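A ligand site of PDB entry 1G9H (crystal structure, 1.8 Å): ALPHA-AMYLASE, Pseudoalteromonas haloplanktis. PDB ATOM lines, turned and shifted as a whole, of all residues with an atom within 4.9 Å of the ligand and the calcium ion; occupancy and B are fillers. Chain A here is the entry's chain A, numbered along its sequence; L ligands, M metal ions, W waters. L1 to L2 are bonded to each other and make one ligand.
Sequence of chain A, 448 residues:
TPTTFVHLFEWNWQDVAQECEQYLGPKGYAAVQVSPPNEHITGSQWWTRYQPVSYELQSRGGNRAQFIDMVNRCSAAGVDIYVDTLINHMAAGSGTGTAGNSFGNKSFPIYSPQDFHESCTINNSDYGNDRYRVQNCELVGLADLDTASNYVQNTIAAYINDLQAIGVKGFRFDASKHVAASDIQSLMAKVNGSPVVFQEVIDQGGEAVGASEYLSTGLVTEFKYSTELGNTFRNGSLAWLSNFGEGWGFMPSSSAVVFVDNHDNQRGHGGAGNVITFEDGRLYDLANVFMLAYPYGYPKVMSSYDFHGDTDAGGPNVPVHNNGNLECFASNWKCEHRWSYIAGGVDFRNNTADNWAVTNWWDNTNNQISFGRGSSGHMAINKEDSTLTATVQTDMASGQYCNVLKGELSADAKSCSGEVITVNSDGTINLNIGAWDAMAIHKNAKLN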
ATOM      1  N   TRP A  46      25.766 -17.400  11.535  1.00  0.00           N
ATOM      2  CA  TRP A  46      24.621 -16.498  11.716  1.00  0.00           C
ATOM      3  C   TRP A  46      23.318 -17.271  11.907  1.00  0.00           C
ATOM      4  O   TRP A  46      22.450 -16.836  12.662  1.00  0.00           O
ATOM      5  CB  TRP A  46      24.478 -15.532  10.523  1.00  0.00           C
ATOM      6  CG  TRP A  46      24.173 -16.234   9.243  1.00  0.00           C
ATOM      7  CD1 TRP A  46      25.081 -16.669   8.334  1.00  0.00           C
ATOM      8  CD2 TRP A  46      22.873 -16.586   8.732  1.00  0.00           C
ATOM      9  NE1 TRP A  46      24.425 -17.291   7.286  1.00  0.00           N
ATOM     10  CE2 TRP A  46      23.079 -17.249   7.504  1.00  0.00           C
ATOM     11  CE3 TRP A  46      21.557 -16.414   9.201  1.00  0.00           C
ATOM     12  CZ2 TRP A  46      22.011 -17.752   6.727  1.00  0.00           C
ATOM     13  CZ3 TRP A  46      20.493 -16.903   8.422  1.00  0.00           C
ATOM     14  CH2 TRP A  46      20.734 -17.566   7.205  1.00  0.00           C
ATOM     15  N   TRP A  47      23.189 -18.419  11.242  1.00  0.00           N
ATOM     16  CA  TRP A  47      21.965 -19.219  11.333  1.00  0.00           C
ATOM     17  C   TRP A  47      21.671 -19.925  12.664  1.00  0.00           C
ATOM     18  O   TRP A  47      20.600 -20.514  12.824  1.00  0.00           O
ATOM     19  CB  TRP A  47      21.827 -20.185  10.143  1.00  0.00           C
ATOM     20  CG  TRP A  47      23.042 -20.962   9.822  1.00  0.00           C
ATOM     21  CD1 TRP A  47      23.872 -20.796   8.751  1.00  0.00           C
ATOM     22  CD2 TRP A  47      23.562 -22.085  10.551  1.00  0.00           C
ATOM     23  NE1 TRP A  47      24.887 -21.730   8.773  1.00  0.00           N
ATOM     24  CE2 TRP A  47      24.712 -22.543   9.867  1.00  0.00           C
ATOM     25  CE3 TRP A  47      23.170 -22.752  11.730  1.00  0.00           C
ATOM     26  CZ2 TRP A  47      25.470 -23.636  10.305  1.00  0.00           C
ATOM     27  CZ3 TRP A  47      23.925 -23.830  12.176  1.00  0.00           C
ATOM     28  CH2 TRP A  47      25.069 -24.260  11.457  1.00  0.00           C
ATOM     29  N   TYR A  50      18.443 -18.934  14.428  1.00  0.00           N
ATOM     30  CA  TYR A  50      17.196 -19.527  13.980  1.00  0.00           C
ATOM     31  C   TYR A  50      16.894 -20.944  14.476  1.00  0.00           C
ATOM     32  O   TYR A  50      16.010 -21.620  13.959  1.00  0.00           O
ATOM     33  CB  TYR A  50      17.108 -19.396  12.462  1.00  0.00           C
ATOM     34  CG  TYR A  50      17.052 -17.931  12.058  1.00  0.00           C
ATOM     35  CD1 TYR A  50      18.209 -17.240  11.701  1.00  0.00           C
ATOM     36  CD2 TYR A  50      15.843 -17.224  12.088  1.00  0.00           C
ATOM     37  CE1 TYR A  50      18.166 -15.865  11.396  1.00  0.00           C
ATOM     38  CE2 TYR A  50      15.782 -15.871  11.802  1.00  0.00           C
ATOM     39  CZ  TYR A  50      16.941 -15.203  11.451  1.00  0.00           C
ATOM     40  OH  TYR A  50      16.863 -13.853  11.179  1.00  0.00           O
ATOM     41  N   LEU A  86      10.386 -16.581  16.127  1.00  0.00           N
ATOM     42  CA  LEU A  86      10.334 -17.927  15.579  1.00  0.00           C
ATOM     43  C   LEU A  86       9.053 -18.626  16.018  1.00  0.00           C
ATOM     44  O   LEU A  86       8.939 -19.092  17.153  1.00  0.00           O
ATOM     45  CB  LEU A  86      11.553 -18.733  16.043  1.00  0.00           C
ATOM     46  CG  LEU A  86      12.946 -18.460  15.460  1.00  0.00           C
ATOM     47  CD1 LEU A  86      13.004 -18.936  14.051  1.00  0.00           C
ATOM     48  CD2 LEU A  86      13.321 -16.995  15.545  1.00  0.00           C
ATOM     49  N   ASN A  88       7.565 -21.146  14.094  1.00  0.00           N
ATOM     50  CA  ASN A  88       7.419 -22.448  13.467  1.00  0.00           C
ATOM     51  C   ASN A  88       8.157 -23.632  14.081  1.00  0.00           C
ATOM     52  O   ASN A  88       7.645 -24.761  14.049  1.00  0.00           O
ATOM     53  CB  ASN A  88       7.834 -22.330  11.986  1.00  0.00           C
ATOM     54  CG  ASN A  88       7.653 -23.628  11.216  1.00  0.00           C
ATOM     55  OD1 ASN A  88       6.528 -24.077  11.000  1.00  0.00           O
ATOM     56  ND2 ASN A  88       8.753 -24.216  10.757  1.00  0.00           N
ATOM     57  N   HIS A  89       9.317 -23.379  14.661  1.00  0.00           N
ATOM     58  CA  HIS A  89      10.133 -24.483  15.138  1.00  0.00           C
ATOM     59  C   HIS A  89      11.061 -24.191  16.307  1.00  0.00           C
ATOM     60  O   HIS A  89      11.146 -23.047  16.803  1.00  0.00           O
ATOM     61  CB  HIS A  89      10.989 -24.938  13.950  1.00  0.00           C
ATOM     62  CG  HIS A  89      11.710 -23.801  13.272  1.00  0.00           C
ATOM     63  ND1 HIS A  89      11.215 -23.178  12.146  1.00  0.00           N
ATOM     64  CD2 HIS A  89      12.850 -23.136  13.590  1.00  0.00           C
ATOM     65  CE1 HIS A  89      12.007 -22.182  11.805  1.00  0.00           C
ATOM     66  NE2 HIS A  89      13.005 -22.137  12.668  1.00  0.00           N
ATOM     67  N   HIS A 117       5.076 -31.850  15.732  1.00  0.00           N
ATOM     68  CA  HIS A 117       4.475 -32.721  14.728  1.00  0.00           C
ATOM     69  C   HIS A 117       5.461 -33.891  14.559  1.00  0.00           C
ATOM     70  O   HIS A 117       6.657 -33.732  14.824  1.00  0.00           O
ATOM     71  CB  HIS A 117       4.374 -31.997  13.378  1.00  0.00           C
ATOM     72  CG  HIS A 117       3.369 -30.898  13.348  1.00  0.00           C
ATOM     73  ND1 HIS A 117       3.630 -29.667  12.785  1.00  0.00           N
ATOM     74  CD2 HIS A 117       2.088 -30.845  13.795  1.00  0.00           C
ATOM     75  CE1 HIS A 117       2.563 -28.900  12.876  1.00  0.00           C
ATOM     76  NE2 HIS A 117       1.613 -29.588  13.491  1.00  0.00           N
ATOM     77  N   TYR A 127       7.026 -27.806  -1.925  1.00  0.00           N
ATOM     78  CA  TYR A 127       6.584 -26.410  -2.060  1.00  0.00           C
ATOM     79  C   TYR A 127       5.550 -26.212  -3.155  1.00  0.00           C
ATOM     80  O   TYR A 127       4.607 -25.438  -2.990  1.00  0.00           O
ATOM     81  CB  TYR A 127       7.782 -25.489  -2.337  1.00  0.00           C
ATOM     82  CG  TYR A 127       8.642 -25.266  -1.134  1.00  0.00           C
ATOM     83  CD1 TYR A 127       9.929 -25.786  -1.064  1.00  0.00           C
ATOM     84  CD2 TYR A 127       8.150 -24.562  -0.031  1.00  0.00           C
ATOM     85  CE1 TYR A 127      10.713 -25.617   0.070  1.00  0.00           C
ATOM     86  CE2 TYR A 127       8.917 -24.388   1.103  1.00  0.00           C
ATOM     87  CZ  TYR A 127      10.203 -24.910   1.149  1.00  0.00           C
ATOM     88  OH  TYR A 127      10.956 -24.743   2.264  1.00  0.00           O
ATOM     89  N   VAL A 134       4.600 -29.031   3.619  1.00  0.00           N
ATOM     90  CA  VAL A 134       5.239 -27.722   3.807  1.00  0.00           C
ATOM     91  C   VAL A 134       4.963 -27.193   5.225  1.00  0.00           C
ATOM     92  O   VAL A 134       5.859 -26.640   5.873  1.00  0.00           O
ATOM     93  CB  VAL A 134       4.723 -26.673   2.738  1.00  0.00           C
ATOM     94  CG1 VAL A 134       5.154 -25.248   3.106  1.00  0.00           C
ATOM     95  CG2 VAL A 134       5.285 -27.009   1.367  1.00  0.00           C
ATOM     96  N   GLN A 135       3.759 -27.430   5.737  1.00  0.00           N
ATOM     97  CA  GLN A 135       3.380 -26.916   7.047  1.00  0.00           C
ATOM     98  C   GLN A 135       3.475 -27.862   8.253  1.00  0.00           C
ATOM     99  O   GLN A 135       3.455 -27.403   9.390  1.00  0.00           O
ATOM    100  CB  GLN A 135       1.982 -26.283   6.967  1.00  0.00           C
ATOM    101  CG  GLN A 135       1.927 -25.195   5.909  1.00  0.00           C
ATOM    102  CD  GLN A 135       0.577 -24.486   5.829  1.00  0.00           C
ATOM    103  OE1 GLN A 135      -0.471 -25.059   6.154  1.00  0.00           O
ATOM    104  NE2 GLN A 135       0.598 -23.216   5.409  1.00  0.00           N
ATOM    105  N   ASN A 136       3.612 -29.169   8.002  1.00  0.00           N
ATOM    106  CA  ASN A 136       3.711 -30.126   9.094  1.00  0.00           C
ATOM    107  C   ASN A 136       5.059 -30.825   9.194  1.00  0.00           C
ATOM    108  O   ASN A 136       5.398 -31.367  10.254  1.00  0.00           O
ATOM    109  CB  ASN A 136       2.562 -31.130   9.038  1.00  0.00           C
ATOM    110  CG  ASN A 136       1.220 -30.465   9.236  1.00  0.00           C
ATOM    111  OD1 ASN A 136       0.876 -30.093  10.349  1.00  0.00           O
ATOM    112  ND2 ASN A 136       0.488 -30.249   8.153  1.00  0.00           N
ATOM    113  N   CYS A 137       5.832 -30.821   8.113  1.00  0.00           N
ATOM    114  CA  CYS A 137       7.152 -31.447   8.144  1.00  0.00           C
ATOM    115  C   CYS A 137       8.237 -30.449   8.544  1.00  0.00           C
ATOM    116  O   CYS A 137       8.000 -29.245   8.686  1.00  0.00           O
ATOM    117  CB  CYS A 137       7.465 -32.137   6.809  1.00  0.00           C
ATOM    118  SG  CYS A 137       6.366 -33.551   6.448  1.00  0.00           S
ATOM    119  N   LEU A 139      11.607 -28.135   8.417  1.00  0.00           N
ATOM    120  CA  LEU A 139      12.386 -27.246   7.556  1.00  0.00           C
ATOM    121  C   LEU A 139      13.850 -27.527   7.931  1.00  0.00           C
ATOM    122  O   LEU A 139      14.308 -27.175   9.026  1.00  0.00           O
ATOM    123  CB  LEU A 139      12.022 -25.780   7.859  1.00  0.00           C
ATOM    124  CG  LEU A 139      12.776 -24.688   7.092  1.00  0.00           C
ATOM    125  CD1 LEU A 139      12.505 -24.833   5.597  1.00  0.00           C
ATOM    126  CD2 LEU A 139      12.359 -23.308   7.608  1.00  0.00           C
ATOM    127  N   LEU A 142      14.627 -28.804  11.469  1.00  0.00           N
ATOM    128  CA  LEU A 142      14.202 -28.029  12.632  1.00  0.00           C
ATOM    129  C   LEU A 142      12.919 -28.637  13.192  1.00  0.00           C
ATOM    130  O   LEU A 142      11.973 -28.881  12.442  1.00  0.00           O
ATOM    131  CB  LEU A 142      14.004 -26.566  12.249  1.00  0.00           C
ATOM    132  CG  LEU A 142      15.289 -25.906  11.714  1.00  0.00           C
ATOM    133  CD1 LEU A 142      14.974 -24.538  11.089  1.00  0.00           C
ATOM    134  CD2 LEU A 142      16.313 -25.773  12.823  1.00  0.00           C
ATOM    135  N   ASP A 144       9.530 -29.266  14.225  1.00  0.00           N
ATOM    136  CA  ASP A 144       8.317 -28.555  13.858  1.00  0.00           C
ATOM    137  C   ASP A 144       7.226 -28.516  14.913  1.00  0.00           C
ATOM    138  O   ASP A 144       6.539 -29.502  15.148  1.00  0.00           O
ATOM    139  CB  ASP A 144       7.782 -29.118  12.548  1.00  0.00           C
ATOM    140  CG  ASP A 144       6.954 -28.110  11.776  1.00  0.00           C
ATOM    141  OD1 ASP A 144       7.506 -27.081  11.341  1.00  0.00           O
ATOM    142  OD2 ASP A 144       5.746 -28.362  11.584  1.00  0.00           O
ATOM    143  N   LEU A 145       7.022 -27.360  15.527  1.00  0.00           N
ATOM    144  CA  LEU A 145       6.008 -27.194  16.577  1.00  0.00           C
ATOM    145  C   LEU A 145       4.582 -27.490  16.131  1.00  0.00           C
ATOM    146  O   LEU A 145       4.195 -27.184  14.988  1.00  0.00           O
ATOM    147  CB  LEU A 145       6.048 -25.777  17.150  1.00  0.00           C
ATOM    148  CG  LEU A 145       7.215 -25.352  18.054  1.00  0.00           C
ATOM    149  CD1 LEU A 145       7.285 -23.828  18.178  1.00  0.00           C
ATOM    150  CD2 LEU A 145       7.042 -26.005  19.410  1.00  0.00           C
ATOM    151  N   ARG A 172       8.421  -9.828  13.479  1.00  0.00           N
ATOM    152  CA  ARG A 172       8.598 -10.475  12.194  1.00  0.00           C
ATOM    153  C   ARG A 172       8.284 -11.934  12.514  1.00  0.00           C
ATOM    154  O   ARG A 172       8.864 -12.486  13.437  1.00  0.00           O
ATOM    155  CB  ARG A 172      10.061 -10.377  11.705  1.00  0.00           C
ATOM    156  CG  ARG A 172      10.323 -11.251  10.477  1.00  0.00           C
ATOM    157  CD  ARG A 172      11.784 -11.277  10.063  1.00  0.00           C
ATOM    158  NE  ARG A 172      12.012 -11.957   8.781  1.00  0.00           N
ATOM    159  CZ  ARG A 172      12.421 -13.215   8.650  1.00  0.00           C
ATOM    160  NH1 ARG A 172      12.602 -13.733   7.433  1.00  0.00           N
ATOM    161  NH2 ARG A 172      12.619 -13.978   9.722  1.00  0.00           N
ATOM    162  N   ASP A 174       8.841 -15.276  11.588  1.00  0.00           N
ATOM    163  CA  ASP A 174       9.732 -16.079  10.764  1.00  0.00           C
ATOM    164  C   ASP A 174       9.078 -17.368  10.264  1.00  0.00           C
ATOM    165  O   ASP A 174       8.258 -17.971  10.951  1.00  0.00           O
ATOM    166  CB  ASP A 174      11.005 -16.411  11.547  1.00  0.00           C
ATOM    167  CG  ASP A 174      11.955 -17.269  10.747  1.00  0.00           C
ATOM    168  OD1 ASP A 174      12.023 -18.486  11.019  1.00  0.00           O
ATOM    169  OD2 ASP A 174      12.608 -16.750   9.822  1.00  0.00           O
ATOM    170  N   ALA A 175       9.431 -17.759   9.041  1.00  0.00           N
ATOM    171  CA  ALA A 175       8.937 -18.980   8.420  1.00  0.00           C
ATOM    172  C   ALA A 175       7.414 -19.128   8.489  1.00  0.00           C
ATOM    173  O   ALA A 175       6.907 -20.235   8.743  1.00  0.00           O
ATOM    174  CB  ALA A 175       9.637 -20.202   9.068  1.00  0.00           C
ATOM    175  N   LYS A 177       5.150 -19.259   6.155  1.00  0.00           N
ATOM    176  CA  LYS A 177       4.601 -20.164   5.154  1.00  0.00           C
ATOM    177  C   LYS A 177       4.470 -21.594   5.711  1.00  0.00           C
ATOM    178  O   LYS A 177       3.618 -22.379   5.285  1.00  0.00           O
ATOM    179  CB  LYS A 177       5.502 -20.218   3.914  1.00  0.00           C
ATOM    180  CG  LYS A 177       4.928 -21.083   2.805  1.00  0.00           C
ATOM    181  CD  LYS A 177       5.966 -21.479   1.774  1.00  0.00           C
ATOM    182  CE  LYS A 177       6.320 -20.319   0.879  1.00  0.00           C
ATOM    183  NZ  LYS A 177       7.390 -20.722  -0.059  1.00  0.00           N
ATOM    184  N   HIS A 178       5.324 -21.900   6.673  1.00  0.00           N
ATOM    185  CA  HIS A 178       5.359 -23.218   7.295  1.00  0.00           C
ATOM    186  C   HIS A 178       4.360 -23.406   8.422  1.00  0.00           C
ATOM    187  O   HIS A 178       4.317 -24.456   9.053  1.00  0.00           O
ATOM    188  CB  HIS A 178       6.791 -23.522   7.726  1.00  0.00           C
ATOM    189  CG  HIS A 178       7.761 -23.481   6.590  1.00  0.00           C
ATOM    190  ND1 HIS A 178       7.945 -24.552   5.741  1.00  0.00           N
ATOM    191  CD2 HIS A 178       8.530 -22.478   6.103  1.00  0.00           C
ATOM    192  CE1 HIS A 178       8.780 -24.210   4.777  1.00  0.00           C
ATOM    193  NE2 HIS A 178       9.156 -22.962   4.972  1.00  0.00           N
ATOM    194  N   VAL A 179       3.537 -22.386   8.641  1.00  0.00           N
ATOM    195  CA  VAL A 179       2.505 -22.443   9.671  1.00  0.00           C
ATOM    196  C   VAL A 179       1.184 -22.077   8.994  1.00  0.00           C
ATOM    197  O   VAL A 179       1.108 -21.087   8.256  1.00  0.00           O
ATOM    198  CB  VAL A 179       2.796 -21.450  10.829  1.00  0.00           C
ATOM    199  CG1 VAL A 179       1.668 -21.486  11.855  1.00  0.00           C
ATOM    200  CG2 VAL A 179       4.125 -21.771  11.464  1.00  0.00           C
ATOM    201  N   GLU A 200       7.016 -13.537   7.101  1.00  0.00           N
ATOM    202  CA  GLU A 200       7.906 -13.945   6.030  1.00  0.00           C
ATOM    203  C   GLU A 200       7.315 -15.087   5.213  1.00  0.00           C
ATOM    204  O   GLU A 200       7.190 -16.226   5.696  1.00  0.00           O
ATOM    205  CB  GLU A 200       9.281 -14.352   6.559  1.00  0.00           C
ATOM    206  CG  GLU A 200      10.256 -14.669   5.436  1.00  0.00           C
ATOM    207  CD  GLU A 200      10.977 -15.995   5.606  1.00  0.00           C
ATOM    208  OE1 GLU A 200      10.550 -16.822   6.442  1.00  0.00           O
ATOM    209  OE2 GLU A 200      11.966 -16.223   4.878  1.00  0.00           O
ATOM    210  N   ILE A 202       7.785 -16.434   1.234  1.00  0.00           N
ATOM    211  CA  ILE A 202       8.429 -16.310  -0.073  1.00  0.00           C
ATOM    212  C   ILE A 202       7.495 -16.903  -1.118  1.00  0.00           C
ATOM    213  O   ILE A 202       7.295 -18.113  -1.167  1.00  0.00           O
ATOM    214  CB  ILE A 202       9.788 -17.031  -0.115  1.00  0.00           C
ATOM    215  CG1 ILE A 202      10.706 -16.466   0.986  1.00  0.00           C
ATOM    216  CG2 ILE A 202      10.424 -16.853  -1.499  1.00  0.00           C
ATOM    217  CD1 ILE A 202      12.040 -17.190   1.191  1.00  0.00           C
ATOM    218  N   GLU A 207       3.326 -21.789  -5.896  1.00  0.00           N
ATOM    219  CA  GLU A 207       3.474 -22.456  -4.603  1.00  0.00           C
ATOM    220  C   GLU A 207       2.122 -23.069  -4.215  1.00  0.00           C
ATOM    221  O   GLU A 207       1.069 -22.575  -4.625  1.00  0.00           O
ATOM    222  CB  GLU A 207       3.871 -21.424  -3.544  1.00  0.00           C
ATOM    223  CG  GLU A 207       5.225 -20.714  -3.738  1.00  0.00           C
ATOM    224  CD  GLU A 207       6.403 -21.562  -3.289  1.00  0.00           C
ATOM    225  OE1 GLU A 207       6.312 -22.193  -2.222  1.00  0.00           O
ATOM    226  OE2 GLU A 207       7.425 -21.578  -4.010  1.00  0.00           O
ATOM    227  N   HIS A 263      18.678 -10.656   4.608  1.00  0.00           N
ATOM    228  CA  HIS A 263      19.783 -11.510   5.049  1.00  0.00           C
ATOM    229  C   HIS A 263      19.888 -12.870   4.349  1.00  0.00           C
ATOM    230  O   HIS A 263      20.985 -13.401   4.198  1.00  0.00           O
ATOM    231  CB  HIS A 263      19.782 -11.671   6.578  1.00  0.00           C
ATOM    232  CG  HIS A 263      18.687 -12.551   7.101  1.00  0.00           C
ATOM    233  ND1 HIS A 263      17.367 -12.184   7.105  1.00  0.00           N
ATOM    234  CD2 HIS A 263      18.730 -13.797   7.638  1.00  0.00           C
ATOM    235  CE1 HIS A 263      16.630 -13.156   7.617  1.00  0.00           C
ATOM    236  NE2 HIS A 263      17.432 -14.145   7.951  1.00  0.00           N
ATOM    237  N   ASP A 264      18.751 -13.434   3.937  1.00  0.00           N
ATOM    238  CA  ASP A 264      18.730 -14.720   3.239  1.00  0.00           C
ATOM    239  C   ASP A 264      19.135 -14.598   1.775  1.00  0.00           C
ATOM    240  O   ASP A 264      20.093 -15.238   1.336  1.00  0.00           O
ATOM    241  CB  ASP A 264      17.335 -15.348   3.257  1.00  0.00           C
ATOM    242  CG  ASP A 264      17.047 -16.142   4.517  1.00  0.00           C
ATOM    243  OD1 ASP A 264      17.982 -16.470   5.271  1.00  0.00           O
ATOM    244  OD2 ASP A 264      15.864 -16.460   4.725  1.00  0.00           O
ATOM    245  N   HIS A 269      19.892 -17.687  -0.592  1.00  0.00           N
ATOM    246  CA  HIS A 269      18.784 -18.476  -0.051  1.00  0.00           C
ATOM    247  C   HIS A 269      17.469 -17.815  -0.433  1.00  0.00           C
ATOM    248  O   HIS A 269      17.129 -16.771   0.112  1.00  0.00           O
ATOM    249  CB  HIS A 269      18.838 -18.554   1.481  1.00  0.00           C
ATOM    250  CG  HIS A 269      20.006 -19.313   2.010  1.00  0.00           C
ATOM    251  ND1 HIS A 269      20.180 -20.669   1.793  1.00  0.00           N
ATOM    252  CD2 HIS A 269      21.096 -18.902   2.715  1.00  0.00           C
ATOM    253  CE1 HIS A 269      21.322 -21.057   2.330  1.00  0.00           C
ATOM    254  NE2 HIS A 269      21.893 -20.005   2.893  1.00  0.00           N
ATOM    255  N   GLY A 270      16.743 -18.426  -1.370  1.00  0.00           N
ATOM    256  CA  GLY A 270      15.466 -17.873  -1.800  1.00  0.00           C
ATOM    257  C   GLY A 270      15.578 -16.763  -2.821  1.00  0.00           C
ATOM    258  O   GLY A 270      14.564 -16.101  -3.127  1.00  0.00           O
HETATM  259  C1  LIG L   1      10.848 -21.415  -1.284  1.00  0.00           C
HETATM  260  C2  LIG L   1      11.031 -20.794   0.083  1.00  0.00           C
HETATM  261  C3  LIG L   1      12.278 -21.370   0.750  1.00  0.00           C
HETATM  262  C4  LIG L   1      13.502 -21.246  -0.165  1.00  0.00           C
HETATM  263  C5  LIG L   1      14.692 -22.011   0.355  1.00  0.00           C
HETATM  264  C6  LIG L   1      12.092 -21.133  -2.093  1.00  0.00           C
HETATM  265  O1  LIG L   1      11.941 -21.665  -3.354  1.00  0.00           O
HETATM  266  O2  LIG L   1       9.731 -20.869  -1.949  1.00  0.00           O
HETATM  267  O3  LIG L   1       9.892 -21.035   0.887  1.00  0.00           O
HETATM  268  O4  LIG L   1      12.532 -20.642   1.946  1.00  0.00           O
HETATM  269  O5  LIG L   1      13.216 -21.765  -1.476  1.00  0.00           O
HETATM  270  O6  LIG L   1      15.846 -21.758  -0.442  1.00  0.00           O
HETATM  271  C1  LG2 L   2      12.726 -21.412   3.100  1.00  0.00           C
HETATM  272  C2  LG2 L   2      11.671 -21.018   4.144  1.00  0.00           C
HETATM  273  O1  LG2 L   2      10.384 -21.025   3.538  1.00  0.00           O
HETATM  274  C3  LG2 L   2      11.955 -19.622   4.716  1.00  0.00           C
HETATM  275  O2  LG2 L   2      11.117 -19.404   5.825  1.00  0.00           O
HETATM  276  C4  LG2 L   2      13.418 -19.495   5.164  1.00  0.00           C
HETATM  277  N1  LG2 L   2      13.827 -18.181   5.628  1.00  0.00           N
HETATM  278  C5  LG2 L   2      14.329 -19.901   4.011  1.00  0.00           C
HETATM  279  O3  LG2 L   2      14.023 -21.248   3.617  1.00  0.00           O
HETATM  280  C6  LG2 L   2      15.793 -19.785   4.414  1.00  0.00           C
HETATM  281  C7  LG2 L   2      13.623 -17.975   7.056  1.00  0.00           C
HETATM  282  C8  LG2 L   2      14.689 -17.071   7.669  1.00  0.00           C
HETATM  283  O4  LG2 L   2      14.758 -15.827   6.973  1.00  0.00           O
HETATM  284  C9  LG2 L   2      16.049 -17.820   7.645  1.00  0.00           C
HETATM  285  O5  LG2 L   2      17.143 -16.935   7.766  1.00  0.00           O
HETATM  286  C10 LG2 L   2      16.060 -18.814   8.823  1.00  0.00           C
HETATM  287  O6  LG2 L   2      17.201 -19.648   8.744  1.00  0.00           O
HETATM  288  C11 LG2 L   2      14.774 -19.630   8.807  1.00  0.00           C
HETATM  289  C12 LG2 L   2      13.583 -19.259   7.946  1.00  0.00           C
HETATM  290  C13 LG2 L   2      14.617 -20.834   9.727  1.00  0.00           C
HETATM  291  O7  LG2 L   2      14.341 -20.169  10.959  1.00  0.00           O
HETATM  292 CA    CA M   1       5.170 -26.062  10.659  1.00  0.00          CA
HETATM  293  O   HOH W   1      13.750 -24.911  -1.960  1.00  0.00           O
HETATM  294  O   HOH W   2       8.321 -18.847   5.146  1.00  0.00           O
HETATM  295  O   HOH W   3       5.244 -25.538  13.069  1.00  0.00           O
HETATM  296  O   HOH W   4       2.903 -25.730  11.764  1.00  0.00           O
HETATM  297  O   HOH W   5      10.731 -18.552  -4.160  1.00  0.00           O
HETATM  298  O   HOH W   6       8.617 -18.928   2.539  1.00  0.00           O
HETATM  299  O   HOH W   7       6.443 -26.837   8.653  1.00  0.00           O
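ND1 of His 178 sits at hydrogen-bond distance from O of Val 134 (3.0 Å).
The backbone NH (N) of Leu 145 is in hydrogen-bond range of the backbone carbonyl oxygen (O) of Asn 88.
NE2 of Gln 135 is in hydrogen-bond range of O of Lys 177, 3.1 Å away.
The backbone carbonyl oxygen of Asp 144 sits at hydrogen-bond distance from the backbone NH of His 117 (2.8 Å).
The side-chain carboxylate (OE2) of Glu 200 is in salt-bridge range of the guanidinium group (NH1) of Arg 172, 3.6 Å away.
The side-chain carboxylate (OE1) of Glu 200 lies within hydrogen-bond range of the backbone NH (N) of Ala 175 (3.0 Å).
A ring nitrogen (NE2) of His 263 lies within hydrogen-bond range of the side-chain hydroxyl (OH) of Tyr 50 (3.3 Å).
OD2 of Asp 174 is in salt-bridge range of NH2 of Arg 172.
OD1 of Asp 174 lies close to O7 of LG2 L2 (2.9 Å).
Residues that only touch the ligand: Tyr 50, Trp 46, Ala 175, Tyr 127, Ile 202, Gly 270, Leu 86, Leu 142 and Leu 139.
Hydrophobic or aromatic side chains within 4 Å of the ligand: Trp 46, Tyr 50, Leu 86, His 89, Tyr 127, Leu 139, Leu 142, Ala 175, His 178, Ile 202 and His 263.
Of the 29 residues printed, 18 come within 4 Å of the ligand.
The nearest printed residue that does not touch the ligand is His 269 (4.3 Å).
The calcium ion is bound by the backbone carbonyl oxygen (O) of His 178, the side-chain amide oxygen (OD1) of Asn 88, water W3, water W7, the backbone carbonyl oxygen (O) of Gln 135, water W4, the side-chain carboxylate (OD2) of Asp 144 and the side-chain carboxylate (OD1) of Asp 144.
The calcium ion has eight donor atoms within binding distance.
NE2 of His 178 lies within hydrogen-bond range of O1 of LG2 L2.
N1 of LG2 L2 lies within salt-bridge range of OD2 of Asp 264, at 2.8 Å.
The side-chain amino group (NZ) of Lys 177 lies within hydrogen-bond range of an oxygen (O3) of LIG L1 (2.7 Å).
OE2 of Glu 200 lies within salt-bridge range of N1 of LG2 L2 (2.8 Å).
NE2 of His 263 sits at hydrogen-bond distance from O5 of LG2 L2.
O7 of LG2 L2 is in hydrogen-bond range of NE2 of His 89 (2.9 Å).
The guanidinium group (NH1) of Arg 172 lies within hydrogen-bond range of an oxygen (O4) of LG2 L2.
The side-chain carboxylate (OE2) of Glu 207 lies within hydrogen-bond range of an oxygen (O2) of LIG L1 (3.2 Å).
Four residues have an atom within 4 Å of the calcium ion: Asn 88, Gln 135, Asp 144 and His 178.
Along chain A the residues within 4 Å of the calcium ion span positions 88 to 178.
The nearest printed residue that does not touch the calcium ion is Asn 136 (4.4 Å).
Water W3 bridges O of Asn 88 (2.7 Å) and O of Leu 145 (2.7 Å).
Water W6 lies within hydrogen-bond range of an oxygen (O1) of LG2 L2, the backbone NH of Ile 202 and the side-chain amino group of Lys 177.
Water W2 lies within hydrogen-bond range of O of Glu 200, O2 of LG2 L2 and N of Lys 177.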
